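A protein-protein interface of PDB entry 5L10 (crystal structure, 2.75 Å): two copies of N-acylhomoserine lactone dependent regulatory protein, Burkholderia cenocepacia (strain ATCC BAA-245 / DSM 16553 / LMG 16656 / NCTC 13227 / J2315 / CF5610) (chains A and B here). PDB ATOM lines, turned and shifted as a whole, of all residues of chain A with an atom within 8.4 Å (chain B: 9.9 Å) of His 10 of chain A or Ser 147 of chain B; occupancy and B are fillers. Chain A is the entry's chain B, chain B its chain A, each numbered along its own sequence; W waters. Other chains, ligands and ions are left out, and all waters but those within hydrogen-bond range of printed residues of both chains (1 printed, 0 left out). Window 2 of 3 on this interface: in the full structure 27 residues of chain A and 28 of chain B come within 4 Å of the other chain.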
ATOM      1  N   ALA A   3      -5.687   3.342   5.202  1.00  0.00           N
ATOM      2  CA  ALA A   3      -5.741   2.258   6.175  1.00  0.00           C
ATOM      3  C   ALA A   3      -4.564   2.339   7.140  1.00  0.00           C
ATOM      4  O   ALA A   3      -4.650   1.853   8.275  1.00  0.00           O
ATOM      5  CB  ALA A   3      -5.763   0.906   5.461  1.00  0.00           C
ATOM      6  N   MET A   4      -3.473   2.978   6.718  1.00  0.00           N
ATOM      7  CA  MET A   4      -2.267   3.120   7.524  1.00  0.00           C
ATOM      8  C   MET A   4      -2.404   4.113   8.674  1.00  0.00           C
ATOM      9  O   MET A   4      -1.885   3.870   9.765  1.00  0.00           O
ATOM     10  CB  MET A   4      -1.100   3.548   6.629  1.00  0.00           C
ATOM     11  CG  MET A   4      -0.562   2.439   5.749  1.00  0.00           C
ATOM     12  SD  MET A   4       0.507   1.174   6.770  1.00  0.00           S
ATOM     13  CE  MET A   4       2.010   2.339   7.200  1.00  0.00           C
ATOM     14  N   ASP A   5      -3.096   5.230   8.415  1.00  0.00           N
ATOM     15  CA  ASP A   5      -3.201   6.306   9.401  1.00  0.00           C
ATOM     16  C   ASP A   5      -3.641   5.785  10.765  1.00  0.00           C
ATOM     17  O   ASP A   5      -3.163   6.258  11.803  1.00  0.00           O
ATOM     18  CB  ASP A   5      -4.170   7.382   8.906  1.00  0.00           C
ATOM     19  CG  ASP A   5      -3.585   8.238   7.793  1.00  0.00           C
ATOM     20  OD1 ASP A   5      -4.130   9.336   7.541  1.00  0.00           O
ATOM     21  OD2 ASP A   5      -2.585   7.820   7.172  1.00  0.00           O
ATOM     22  N   LEU A   6      -4.545   4.801  10.787  1.00  0.00           N
ATOM     23  CA  LEU A   6      -4.980   4.243  12.062  1.00  0.00           C
ATOM     24  C   LEU A   6      -3.907   3.345  12.667  1.00  0.00           C
ATOM     25  O   LEU A   6      -3.750   3.295  13.892  1.00  0.00           O
ATOM     26  CB  LEU A   6      -6.287   3.475  11.887  1.00  0.00           C
ATOM     27  CG  LEU A   6      -7.148   3.432  13.148  1.00  0.00           C
ATOM     28  CD1 LEU A   6      -7.461   4.852  13.604  1.00  0.00           C
ATOM     29  CD2 LEU A   6      -8.422   2.650  12.899  1.00  0.00           C
ATOM     30  N   THR A   7      -3.163   2.622  11.826  1.00  0.00           N
ATOM     31  CA  THR A   7      -2.056   1.818  12.333  1.00  0.00           C
ATOM     32  C   THR A   7      -0.825   2.670  12.620  1.00  0.00           C
ATOM     33  O   THR A   7      -0.044   2.336  13.519  1.00  0.00           O
ATOM     34  CB  THR A   7      -1.707   0.701  11.345  1.00  0.00           C
ATOM     35  OG1 THR A   7      -1.287   1.271  10.099  1.00  0.00           O
ATOM     36  CG2 THR A   7      -2.914  -0.202  11.106  1.00  0.00           C
ATOM     37  N   ILE A   8      -0.635   3.763  11.872  1.00  0.00           N
ATOM     38  CA  ILE A   8       0.427   4.713  12.195  1.00  0.00           C
ATOM     39  C   ILE A   8       0.243   5.240  13.613  1.00  0.00           C
ATOM     40  O   ILE A   8       1.187   5.285  14.410  1.00  0.00           O
ATOM     41  CB  ILE A   8       0.456   5.861  11.169  1.00  0.00           C
ATOM     42  CG1 ILE A   8       0.884   5.349   9.792  1.00  0.00           C
ATOM     43  CG2 ILE A   8       1.388   6.976  11.632  1.00  0.00           C
ATOM     44  CD1 ILE A   8       0.753   6.383   8.689  1.00  0.00           C
ATOM     45  N   LEU A   9      -0.986   5.637  13.951  1.00  0.00           N
ATOM     46  CA  LEU A   9      -1.248   6.155  15.287  1.00  0.00           C
ATOM     47  C   LEU A   9      -1.291   5.042  16.323  1.00  0.00           C
ATOM     48  O   LEU A   9      -0.872   5.249  17.467  1.00  0.00           O
ATOM     49  CB  LEU A   9      -2.558   6.939  15.299  1.00  0.00           C
ATOM     50  CG  LEU A   9      -2.598   8.185  14.413  1.00  0.00           C
ATOM     51  CD1 LEU A   9      -4.002   8.757  14.385  1.00  0.00           C
ATOM     52  CD2 LEU A   9      -1.597   9.225  14.896  1.00  0.00           C
ATOM     53  N   HIS A  10      -1.790   3.862  15.946  1.00  0.00           N
ATOM     54  CA  HIS A  10      -1.826   2.745  16.884  1.00  0.00           C
ATOM     55  C   HIS A  10      -0.425   2.407  17.377  1.00  0.00           C
ATOM     56  O   HIS A  10      -0.206   2.212  18.578  1.00  0.00           O
ATOM     57  CB  HIS A  10      -2.478   1.527  16.231  1.00  0.00           C
ATOM     58  CG  HIS A  10      -2.782   0.420  17.191  1.00  0.00           C
ATOM     59  ND1 HIS A  10      -3.061  -0.866  16.780  1.00  0.00           N
ATOM     60  CD2 HIS A  10      -2.860   0.406  18.542  1.00  0.00           C
ATOM     61  CE1 HIS A  10      -3.292  -1.625  17.836  1.00  0.00           C
ATOM     62  NE2 HIS A  10      -3.176  -0.877  18.919  1.00  0.00           N
ATOM     63  N   ASP A  11       0.544   2.350  16.459  1.00  0.00           N
ATOM     64  CA  ASP A  11       1.919   2.057  16.849  1.00  0.00           C
ATOM     65  C   ASP A  11       2.489   3.159  17.731  1.00  0.00           C
ATOM     66  O   ASP A  11       3.245   2.886  18.671  1.00  0.00           O
ATOM     67  CB  ASP A  11       2.788   1.862  15.608  1.00  0.00           C
ATOM     68  CG  ASP A  11       2.422   0.614  14.832  1.00  0.00           C
ATOM     69  OD1 ASP A  11       1.830  -0.310  15.433  1.00  0.00           O
ATOM     70  OD2 ASP A  11       2.733   0.553  13.624  1.00  0.00           O
ATOM     71  N   CYS A  12       2.135   4.412  17.441  1.00  0.00           N
ATOM     72  CA  CYS A  12       2.578   5.526  18.272  1.00  0.00           C
ATOM     73  C   CYS A  12       2.044   5.401  19.694  1.00  0.00           C
ATOM     74  O   CYS A  12       2.797   5.541  20.665  1.00  0.00           O
ATOM     75  CB  CYS A  12       2.133   6.847  17.650  1.00  0.00           C
ATOM     76  SG  CYS A  12       2.401   8.282  18.704  1.00  0.00           S
ATOM     77  N   PHE A  13       0.744   5.140  19.839  1.00  0.00           N
ATOM     78  CA  PHE A  13       0.155   5.124  21.172  1.00  0.00           C
ATOM     79  C   PHE A  13       0.622   3.925  21.987  1.00  0.00           C
ATOM     80  O   PHE A  13       0.709   4.017  23.217  1.00  0.00           O
ATOM     81  CB  PHE A  13      -1.369   5.158  21.071  1.00  0.00           C
ATOM     82  CG  PHE A  13      -1.932   6.548  20.991  1.00  0.00           C
ATOM     83  CD1 PHE A  13      -2.320   7.217  22.141  1.00  0.00           C
ATOM     84  CD2 PHE A  13      -2.051   7.197  19.772  1.00  0.00           C
ATOM     85  CE1 PHE A  13      -2.831   8.506  22.076  1.00  0.00           C
ATOM     86  CE2 PHE A  13      -2.561   8.484  19.699  1.00  0.00           C
ATOM     87  CZ  PHE A  13      -2.950   9.139  20.854  1.00  0.00           C
ATOM     88  N   ASP A  14       0.940   2.807  21.325  1.00  0.00           N
ATOM     89  CA  ASP A  14       1.540   1.673  22.021  1.00  0.00           C
ATOM     90  C   ASP A  14       2.917   2.030  22.576  1.00  0.00           C
ATOM     91  O   ASP A  14       3.228   1.716  23.731  1.00  0.00           O
ATOM     92  CB  ASP A  14       1.630   0.466  21.083  1.00  0.00           C
ATOM     93  CG  ASP A  14       0.311  -0.293  20.975  1.00  0.00           C
ATOM     94  OD1 ASP A  14      -0.726   0.326  20.660  1.00  0.00           O
ATOM     95  OD2 ASP A  14       0.318  -1.518  21.208  1.00  0.00           O
ATOM     96  N   ALA A  15       3.753   2.698  21.773  1.00  0.00           N
ATOM     97  CA  ALA A  15       5.087   3.073  22.239  1.00  0.00           C
ATOM     98  C   ALA A  15       5.030   4.055  23.405  1.00  0.00           C
ATOM     99  O   ALA A  15       5.882   4.006  24.303  1.00  0.00           O
ATOM    100  CB  ALA A  15       5.901   3.668  21.089  1.00  0.00           C
ATOM    101  N   LEU A  16       4.035   4.944  23.420  1.00  0.00           N
ATOM    102  CA  LEU A  16       3.936   5.942  24.480  1.00  0.00           C
ATOM    103  C   LEU A  16       3.487   5.354  25.811  1.00  0.00           C
ATOM    104  O   LEU A  16       3.616   6.029  26.839  1.00  0.00           O
ATOM    105  CB  LEU A  16       2.982   7.061  24.060  1.00  0.00           C
ATOM    106  CG  LEU A  16       3.479   7.900  22.876  1.00  0.00           C
ATOM    107  CD1 LEU A  16       2.422   8.881  22.392  1.00  0.00           C
ATOM    108  CD2 LEU A  16       4.756   8.631  23.249  1.00  0.00           C
ATOM    109  N   GLN A  17       2.965   4.126  25.821  1.00  0.00           N
ATOM    110  CA  GLN A  17       2.605   3.491  27.084  1.00  0.00           C
ATOM    111  C   GLN A  17       3.847   3.104  27.876  1.00  0.00           C
ATOM    112  O   GLN A  17       3.849   3.169  29.111  1.00  0.00           O
ATOM    113  CB  GLN A  17       1.730   2.266  26.827  1.00  0.00           C
ATOM    114  CG  GLN A  17       0.434   2.577  26.100  1.00  0.00           C
ATOM    115  CD  GLN A  17      -0.390   3.636  26.809  1.00  0.00           C
ATOM    116  OE1 GLN A  17      -0.707   3.503  27.993  1.00  0.00           O
ATOM    117  NE2 GLN A  17      -0.740   4.696  26.088  1.00  0.00           N
ATOM    118  N   ARG A  18       4.907   2.699  27.186  1.00  0.00           N
ATOM    119  CA  ARG A  18       6.171   2.322  27.818  1.00  0.00           C
ATOM    120  C   ARG A  18       7.245   3.365  27.506  1.00  0.00           C
ATOM    121  O   ARG A  18       8.301   3.071  26.935  1.00  0.00           O
ATOM    122  CB  ARG A  18       6.588   0.925  27.357  1.00  0.00           C
ATOM    123  CG  ARG A  18       6.321   0.680  25.879  1.00  0.00           C
ATOM    124  CD  ARG A  18       6.871  -0.653  25.389  1.00  0.00           C
ATOM    125  NE  ARG A  18       6.485  -0.899  24.001  1.00  0.00           N
ATOM    126  CZ  ARG A  18       7.102  -0.375  22.945  1.00  0.00           C
ATOM    127  NH1 ARG A  18       8.145   0.429  23.110  1.00  0.00           N
ATOM    128  NH2 ARG A  18       6.675  -0.652  21.719  1.00  0.00           N
ATOM    129  N   PRO A  28       8.296   8.509  19.145  1.00  0.00           N
ATOM    130  CA  PRO A  28       7.079   7.926  18.545  1.00  0.00           C
ATOM    131  C   PRO A  28       6.144   8.970  17.963  1.00  0.00           C
ATOM    132  O   PRO A  28       5.534   8.738  16.912  1.00  0.00           O
ATOM    133  CB  PRO A  28       6.428   7.174  19.716  1.00  0.00           C
ATOM    134  CG  PRO A  28       7.525   6.938  20.671  1.00  0.00           C
ATOM    135  CD  PRO A  28       8.393   8.147  20.572  1.00  0.00           C
ATOM    136  N   ALA A  32       5.297   9.351  13.937  1.00  0.00           N
ATOM    137  CA  ALA A  32       3.955   9.436  13.374  1.00  0.00           C
ATOM    138  C   ALA A  32       3.806  10.672  12.497  1.00  0.00           C
ATOM    139  O   ALA A  32       3.255  10.599  11.393  1.00  0.00           O
ATOM    140  CB  ALA A  32       2.913   9.440  14.492  1.00  0.00           C
ATOM    141  N   SER A 155      -5.193  13.292  17.194  1.00  0.00           N
ATOM    142  CA  SER A 155      -4.604  12.261  18.041  1.00  0.00           C
ATOM    143  C   SER A 155      -3.180  12.618  18.433  1.00  0.00           C
ATOM    144  O   SER A 155      -2.773  12.407  19.581  1.00  0.00           O
ATOM    145  CB  SER A 155      -4.631  10.910  17.330  1.00  0.00           C
ATOM    146  OG  SER A 155      -5.958  10.512  17.054  1.00  0.00           O
ATOM    147  N   ASN B   2     -11.858  -2.296  10.832  1.00  0.00           N
ATOM    148  CA  ASN B   2     -11.256  -1.328  11.740  1.00  0.00           C
ATOM    149  C   ASN B   2     -10.860  -0.052  11.001  1.00  0.00           C
ATOM    150  O   ASN B   2     -10.793   1.018  11.599  1.00  0.00           O
ATOM    151  CB  ASN B   2     -10.041  -1.934  12.444  1.00  0.00           C
ATOM    152  CG  ASN B   2      -8.939  -2.321  11.479  1.00  0.00           C
ATOM    153  OD1 ASN B   2      -9.195  -2.591  10.305  1.00  0.00           O
ATOM    154  ND2 ASN B   2      -7.706  -2.352  11.969  1.00  0.00           N
ATOM    155  N   ASP B   5     -13.103   2.843  11.462  1.00  0.00           N
ATOM    156  CA  ASP B   5     -12.939   3.754  12.592  1.00  0.00           C
ATOM    157  C   ASP B   5     -12.387   5.102  12.145  1.00  0.00           C
ATOM    158  O   ASP B   5     -12.794   6.149  12.659  1.00  0.00           O
ATOM    159  CB  ASP B   5     -12.024   3.130  13.650  1.00  0.00           C
ATOM    160  CG  ASP B   5     -12.551   1.807  14.181  1.00  0.00           C
ATOM    161  OD1 ASP B   5     -13.696   1.435  13.845  1.00  0.00           O
ATOM    162  OD2 ASP B   5     -11.820   1.143  14.946  1.00  0.00           O
ATOM    163  N   LEU B   6     -11.455   5.096  11.189  1.00  0.00           N
ATOM    164  CA  LEU B   6     -10.896   6.354  10.706  1.00  0.00           C
ATOM    165  C   LEU B   6     -11.911   7.141   9.888  1.00  0.00           C
ATOM    166  O   LEU B   6     -11.901   8.378   9.911  1.00  0.00           O
ATOM    167  CB  LEU B   6      -9.634   6.090   9.887  1.00  0.00           C
ATOM    168  CG  LEU B   6      -8.922   7.348   9.387  1.00  0.00           C
ATOM    169  CD1 LEU B   6      -8.584   8.278  10.548  1.00  0.00           C
ATOM    170  CD2 LEU B   6      -7.678   6.976   8.609  1.00  0.00           C
ATOM    171  N   VAL B  93      -9.676   5.081  32.487  1.00  0.00           N
ATOM    172  CA  VAL B  93     -10.618   3.995  32.234  1.00  0.00           C
ATOM    173  C   VAL B  93     -11.143   3.506  33.576  1.00  0.00           C
ATOM    174  O   VAL B  93     -10.358   3.218  34.489  1.00  0.00           O
ATOM    175  CB  VAL B  93      -9.953   2.849  31.454  1.00  0.00           C
ATOM    176  CG1 VAL B  93     -10.957   1.743  31.163  1.00  0.00           C
ATOM    177  CG2 VAL B  93      -9.333   3.374  30.172  1.00  0.00           C
ATOM    178  N   TRP B 118     -14.627   5.738  29.726  1.00  0.00           N
ATOM    179  CA  TRP B 118     -13.351   6.300  29.300  1.00  0.00           C
ATOM    180  C   TRP B 118     -13.486   7.808  29.465  1.00  0.00           C
ATOM    181  O   TRP B 118     -14.345   8.426  28.826  1.00  0.00           O
ATOM    182  CB  TRP B 118     -13.050   5.913  27.850  1.00  0.00           C
ATOM    183  CG  TRP B 118     -11.737   6.381  27.301  1.00  0.00           C
ATOM    184  CD1 TRP B 118     -10.590   5.653  27.198  1.00  0.00           C
ATOM    185  CD2 TRP B 118     -11.445   7.672  26.749  1.00  0.00           C
ATOM    186  NE1 TRP B 118      -9.595   6.412  26.630  1.00  0.00           N
ATOM    187  CE2 TRP B 118     -10.094   7.655  26.344  1.00  0.00           C
ATOM    188  CE3 TRP B 118     -12.190   8.840  26.562  1.00  0.00           C
ATOM    189  CZ2 TRP B 118      -9.470   8.766  25.763  1.00  0.00           C
ATOM    190  CZ3 TRP B 118     -11.571   9.944  25.984  1.00  0.00           C
ATOM    191  CH2 TRP B 118     -10.223   9.896  25.591  1.00  0.00           C
ATOM    192  N   LEU B 141     -14.071  -2.878  28.358  1.00  0.00           N
ATOM    193  CA  LEU B 141     -13.106  -3.132  27.294  1.00  0.00           C
ATOM    194  C   LEU B 141     -11.928  -3.948  27.814  1.00  0.00           C
ATOM    195  O   LEU B 141     -11.345  -3.623  28.853  1.00  0.00           O
ATOM    196  CB  LEU B 141     -12.608  -1.816  26.699  1.00  0.00           C
ATOM    197  CG  LEU B 141     -13.593  -0.987  25.875  1.00  0.00           C
ATOM    198  CD1 LEU B 141     -13.073   0.430  25.673  1.00  0.00           C
ATOM    199  CD2 LEU B 141     -13.836  -1.655  24.537  1.00  0.00           C
ATOM    200  N   ASP B 142     -11.579  -5.012  27.092  1.00  0.00           N
ATOM    201  CA  ASP B 142     -10.324  -5.694  27.368  1.00  0.00           C
ATOM    202  C   ASP B 142      -9.159  -4.842  26.879  1.00  0.00           C
ATOM    203  O   ASP B 142      -9.318  -3.948  26.044  1.00  0.00           O
ATOM    204  CB  ASP B 142     -10.287  -7.079  26.713  1.00  0.00           C
ATOM    205  CG  ASP B 142     -10.542  -7.028  25.219  1.00  0.00           C
ATOM    206  OD1 ASP B 142     -11.676  -6.690  24.828  1.00  0.00           O
ATOM    207  OD2 ASP B 142      -9.619  -7.341  24.436  1.00  0.00           O
ATOM    208  N   ALA B 143      -7.973  -5.132  27.417  1.00  0.00           N
ATOM    209  CA  ALA B 143      -6.795  -4.329  27.101  1.00  0.00           C
ATOM    210  C   ALA B 143      -6.516  -4.283  25.603  1.00  0.00           C
ATOM    211  O   ALA B 143      -6.022  -3.269  25.096  1.00  0.00           O
ATOM    212  CB  ALA B 143      -5.579  -4.873  27.850  1.00  0.00           C
ATOM    213  N   ASP B 144      -6.824  -5.363  24.882  1.00  0.00           N
ATOM    214  CA  ASP B 144      -6.591  -5.385  23.442  1.00  0.00           C
ATOM    215  C   ASP B 144      -7.519  -4.424  22.709  1.00  0.00           C
ATOM    216  O   ASP B 144      -7.126  -3.841  21.692  1.00  0.00           O
ATOM    217  CB  ASP B 144      -6.761  -6.809  22.913  1.00  0.00           C
ATOM    218  CG  ASP B 144      -5.950  -7.067  21.659  1.00  0.00           C
ATOM    219  OD1 ASP B 144      -4.706  -7.119  21.759  1.00  0.00           O
ATOM    220  OD2 ASP B 144      -6.556  -7.235  20.579  1.00  0.00           O
ATOM    221  N   GLU B 145      -8.749  -4.250  23.202  1.00  0.00           N
ATOM    222  CA  GLU B 145      -9.647  -3.259  22.617  1.00  0.00           C
ATOM    223  C   GLU B 145      -9.251  -1.847  23.029  1.00  0.00           C
ATOM    224  O   GLU B 145      -9.415  -0.899  22.253  1.00  0.00           O
ATOM    225  CB  GLU B 145     -11.093  -3.544  23.024  1.00  0.00           C
ATOM    226  CG  GLU B 145     -11.770  -4.658  22.241  1.00  0.00           C
ATOM    227  CD  GLU B 145     -13.205  -4.889  22.688  1.00  0.00           C
ATOM    228  OE1 GLU B 145     -13.472  -4.777  23.904  1.00  0.00           O
ATOM    229  OE2 GLU B 145     -14.067  -5.170  21.828  1.00  0.00           O
ATOM    230  N   ILE B 146      -8.741  -1.689  24.253  1.00  0.00           N
ATOM    231  CA  ILE B 146      -8.259  -0.382  24.689  1.00  0.00           C
ATOM    232  C   ILE B 146      -7.096   0.071  23.817  1.00  0.00           C
ATOM    233  O   ILE B 146      -7.036   1.228  23.386  1.00  0.00           O
ATOM    234  CB  ILE B 146      -7.864  -0.424  26.177  1.00  0.00           C
ATOM    235  CG1 ILE B 146      -9.078  -0.756  27.041  1.00  0.00           C
ATOM    236  CG2 ILE B 146      -7.260   0.903  26.601  1.00  0.00           C
ATOM    237  CD1 ILE B 146      -8.761  -0.856  28.514  1.00  0.00           C
ATOM    238  N   SER B 147      -6.163  -0.842  23.532  1.00  0.00           N
ATOM    239  CA  SER B 147      -5.006  -0.501  22.711  1.00  0.00           C
ATOM    240  C   SER B 147      -5.426   0.053  21.354  1.00  0.00           C
ATOM    241  O   SER B 147      -4.879   1.061  20.891  1.00  0.00           O
ATOM    242  CB  SER B 147      -4.115  -1.732  22.539  1.00  0.00           C
ATOM    243  OG  SER B 147      -3.188  -1.550  21.484  1.00  0.00           O
ATOM    244  N   ARG B 148      -6.406  -0.581  20.710  1.00  0.00           N
ATOM    245  CA  ARG B 148      -6.834  -0.143  19.388  1.00  0.00           C
ATOM    246  C   ARG B 148      -7.703   1.108  19.433  1.00  0.00           C
ATOM    247  O   ARG B 148      -7.806   1.810  18.420  1.00  0.00           O
ATOM    248  CB  ARG B 148      -7.571  -1.282  18.675  1.00  0.00           C
ATOM    249  CG  ARG B 148      -9.060  -1.066  18.499  1.00  0.00           C
ATOM    250  CD  ARG B 148      -9.850  -2.247  19.031  1.00  0.00           C
ATOM    251  NE  ARG B 148     -11.291  -2.017  18.966  1.00  0.00           N
ATOM    252  CZ  ARG B 148     -12.132  -2.733  18.226  1.00  0.00           C
ATOM    253  NH1 ARG B 148     -11.680  -3.739  17.490  1.00  0.00           N
ATOM    254  NH2 ARG B 148     -13.428  -2.447  18.233  1.00  0.00           N
ATOM    255  N   LEU B 149      -8.303   1.422  20.582  1.00  0.00           N
ATOM    256  CA  LEU B 149      -9.180   2.581  20.710  1.00  0.00           C
ATOM    257  C   LEU B 149      -8.478   3.825  21.235  1.00  0.00           C
ATOM    258  O   LEU B 149      -9.116   4.880  21.310  1.00  0.00           O
ATOM    259  CB  LEU B 149     -10.357   2.261  21.634  1.00  0.00           C
ATOM    260  CG  LEU B 149     -11.549   1.514  21.042  1.00  0.00           C
ATOM    261  CD1 LEU B 149     -12.632   1.369  22.092  1.00  0.00           C
ATOM    262  CD2 LEU B 149     -12.080   2.244  19.823  1.00  0.00           C
ATOM    263  N   ARG B 150      -7.198   3.736  21.605  1.00  0.00           N
ATOM    264  CA  ARG B 150      -6.509   4.897  22.162  1.00  0.00           C
ATOM    265  C   ARG B 150      -6.489   6.053  21.173  1.00  0.00           C
ATOM    266  O   ARG B 150      -6.937   7.163  21.488  1.00  0.00           O
ATOM    267  CB  ARG B 150      -5.087   4.521  22.576  1.00  0.00           C
ATOM    268  CG  ARG B 150      -5.005   3.874  23.934  1.00  0.00           C
ATOM    269  CD  ARG B 150      -3.608   3.981  24.513  1.00  0.00           C
ATOM    270  NE  ARG B 150      -3.544   3.354  25.828  1.00  0.00           N
ATOM    271  CZ  ARG B 150      -3.198   2.089  26.033  1.00  0.00           C
ATOM    272  NH1 ARG B 150      -2.870   1.313  25.008  1.00  0.00           N
ATOM    273  NH2 ARG B 150      -3.173   1.601  27.266  1.00  0.00           N
ATOM    274  N   ALA B 151      -5.972   5.813  19.969  1.00  0.00           N
ATOM    275  CA  ALA B 151      -5.912   6.869  18.959  1.00  0.00           C
ATOM    276  C   ALA B 151      -7.283   7.432  18.606  1.00  0.00           C
ATOM    277  O   ALA B 151      -7.422   8.667  18.568  1.00  0.00           O
ATOM    278  CB  ALA B 151      -5.181   6.353  17.717  1.00  0.00           C
ATOM    279  N   PRO B 152      -8.320   6.625  18.331  1.00  0.00           N
ATOM    280  CA  PRO B 152      -9.633   7.234  18.046  1.00  0.00           C
ATOM    281  C   PRO B 152     -10.200   8.017  19.216  1.00  0.00           C
ATOM    282  O   PRO B 152     -10.733   9.116  19.020  1.00  0.00           O
ATOM    283  CB  PRO B 152     -10.508   6.024  17.691  1.00  0.00           C
ATOM    284  CG  PRO B 152      -9.546   4.993  17.229  1.00  0.00           C
ATOM    285  CD  PRO B 152      -8.346   5.170  18.097  1.00  0.00           C
ATOM    286  N   CYS B 153     -10.106   7.483  20.435  1.00  0.00           N
ATOM    287  CA  CYS B 153     -10.617   8.213  21.591  1.00  0.00           C
ATOM    288  C   CYS B 153      -9.846   9.505  21.810  1.00  0.00           C
ATOM    289  O   CYS B 153     -10.433  10.530  22.178  1.00  0.00           O
ATOM    290  CB  CYS B 153     -10.557   7.333  22.835  1.00  0.00           C
ATOM    291  SG  CYS B 153     -11.838   6.083  22.882  1.00  0.00           S
ATOM    292  N   ALA B 154      -8.527   9.470  21.602  1.00  0.00           N
ATOM    293  CA  ALA B 154      -7.721  10.685  21.656  1.00  0.00           C
ATOM    294  C   ALA B 154      -8.238  11.719  20.667  1.00  0.00           C
ATOM    295  O   ALA B 154      -8.373  12.904  20.995  1.00  0.00           O
ATOM    296  CB  ALA B 154      -6.261  10.347  21.359  1.00  0.00           C
HETATM  297  O   HOH W   1      -2.382   1.844  22.292  1.00  0.00           O
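Of the 19 printed residues of chain B, 8 touch a printed residue of chain A. Hydrophobic or aromatic side chains of chain B within 4 Å of the printed part of chain A: Leu 6, Ala 151 and Ala 154. Of the 19 printed residues of chain A, 8 touch a printed residue of chain B.
Water W1 lies within hydrogen-bond range of OD1 of Asp 14 of chain A (2.8 Å), NH1 of Arg 150 of chain B (2.8 Å) and O of Ser 147 of chain B (3.0 Å).
His 10 of chain A touches just these residues of chain B: Ser 147 and Arg 148. Printed residues of chain B within 4 Å of Phe 13 of chain A: Arg 150 (3.9 Å), Ala 151 (3.8 Å) and Ala 154 (3.6 Å). Of the printed residues of chain B, Gln 17 of chain A touches Arg 150 (3.1 Å). Of chain A, only His 10 and Asp 14 come within 4 Å of Ser 147 of chain B. Printed residues of chain A within 4 Å of Ala 154 of chain B: Phe 13 (3.6 Å).
Asp 5 of chain A touches Leu 6 of chain B, and with the chains exchanged Leu 6 of chain A touches Asp 5 of chain B. Of the 12 pairs that touch across the chains among the printed residues, 2 have their exchanged pair printed and touching as well.
Among the printed residues, pairs that only touch across the chains: Asp 5 of chain A with Leu 6 of chain B (3.5 Å), Leu 6 of chain A with Asn 2 of chain B (3.2 Å), Leu 6 of chain A with Asp 5 of chain B (3.7 Å), Leu 9 of chain A with Ala 151 of chain B (3.6 Å), His 10 of chain A with Arg 148 of chain B (3.7 Å), Phe 13 of chain A with Arg 150 of chain B (3.9 Å), Phe 13 of chain A with Ala 151 of chain B (3.8 Å) and Phe 13 of chain A with Ala 154 of chain B (3.6 Å).
A ring nitrogen (NE2) of His 10 of chain A sits close to the side-chain carboxylate (OD1) of Asp 14 of chain A, 3.2 Å away. The backbone carbonyl oxygen of Phe 13 of chain A sits close to the side-chain amide nitrogen of Gln 17 of chain A, 3.3 Å away.
The backbone carbonyl oxygen of Ala 151 of chain B lies within hydrogen-bond range of the side-chain hydroxyl of Ser 155 of chain A (2.8 Å). The side-chain hydroxyl (OG) of Ser 147 of chain B sits at hydrogen-bond distance from a ring nitrogen (NE2) of His 10 of chain A. The side-chain amide nitrogen (NE2) of Gln 17 of chain A sits close to the guanidinium group (NE) of Arg 150 of chain B (3.1 Å). The side-chain hydroxyl (OG) of Ser 147 of chain B is in hydrogen-bond range of the side-chain carboxylate (OD1) of Asp 14 of chain A (3.2 Å).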
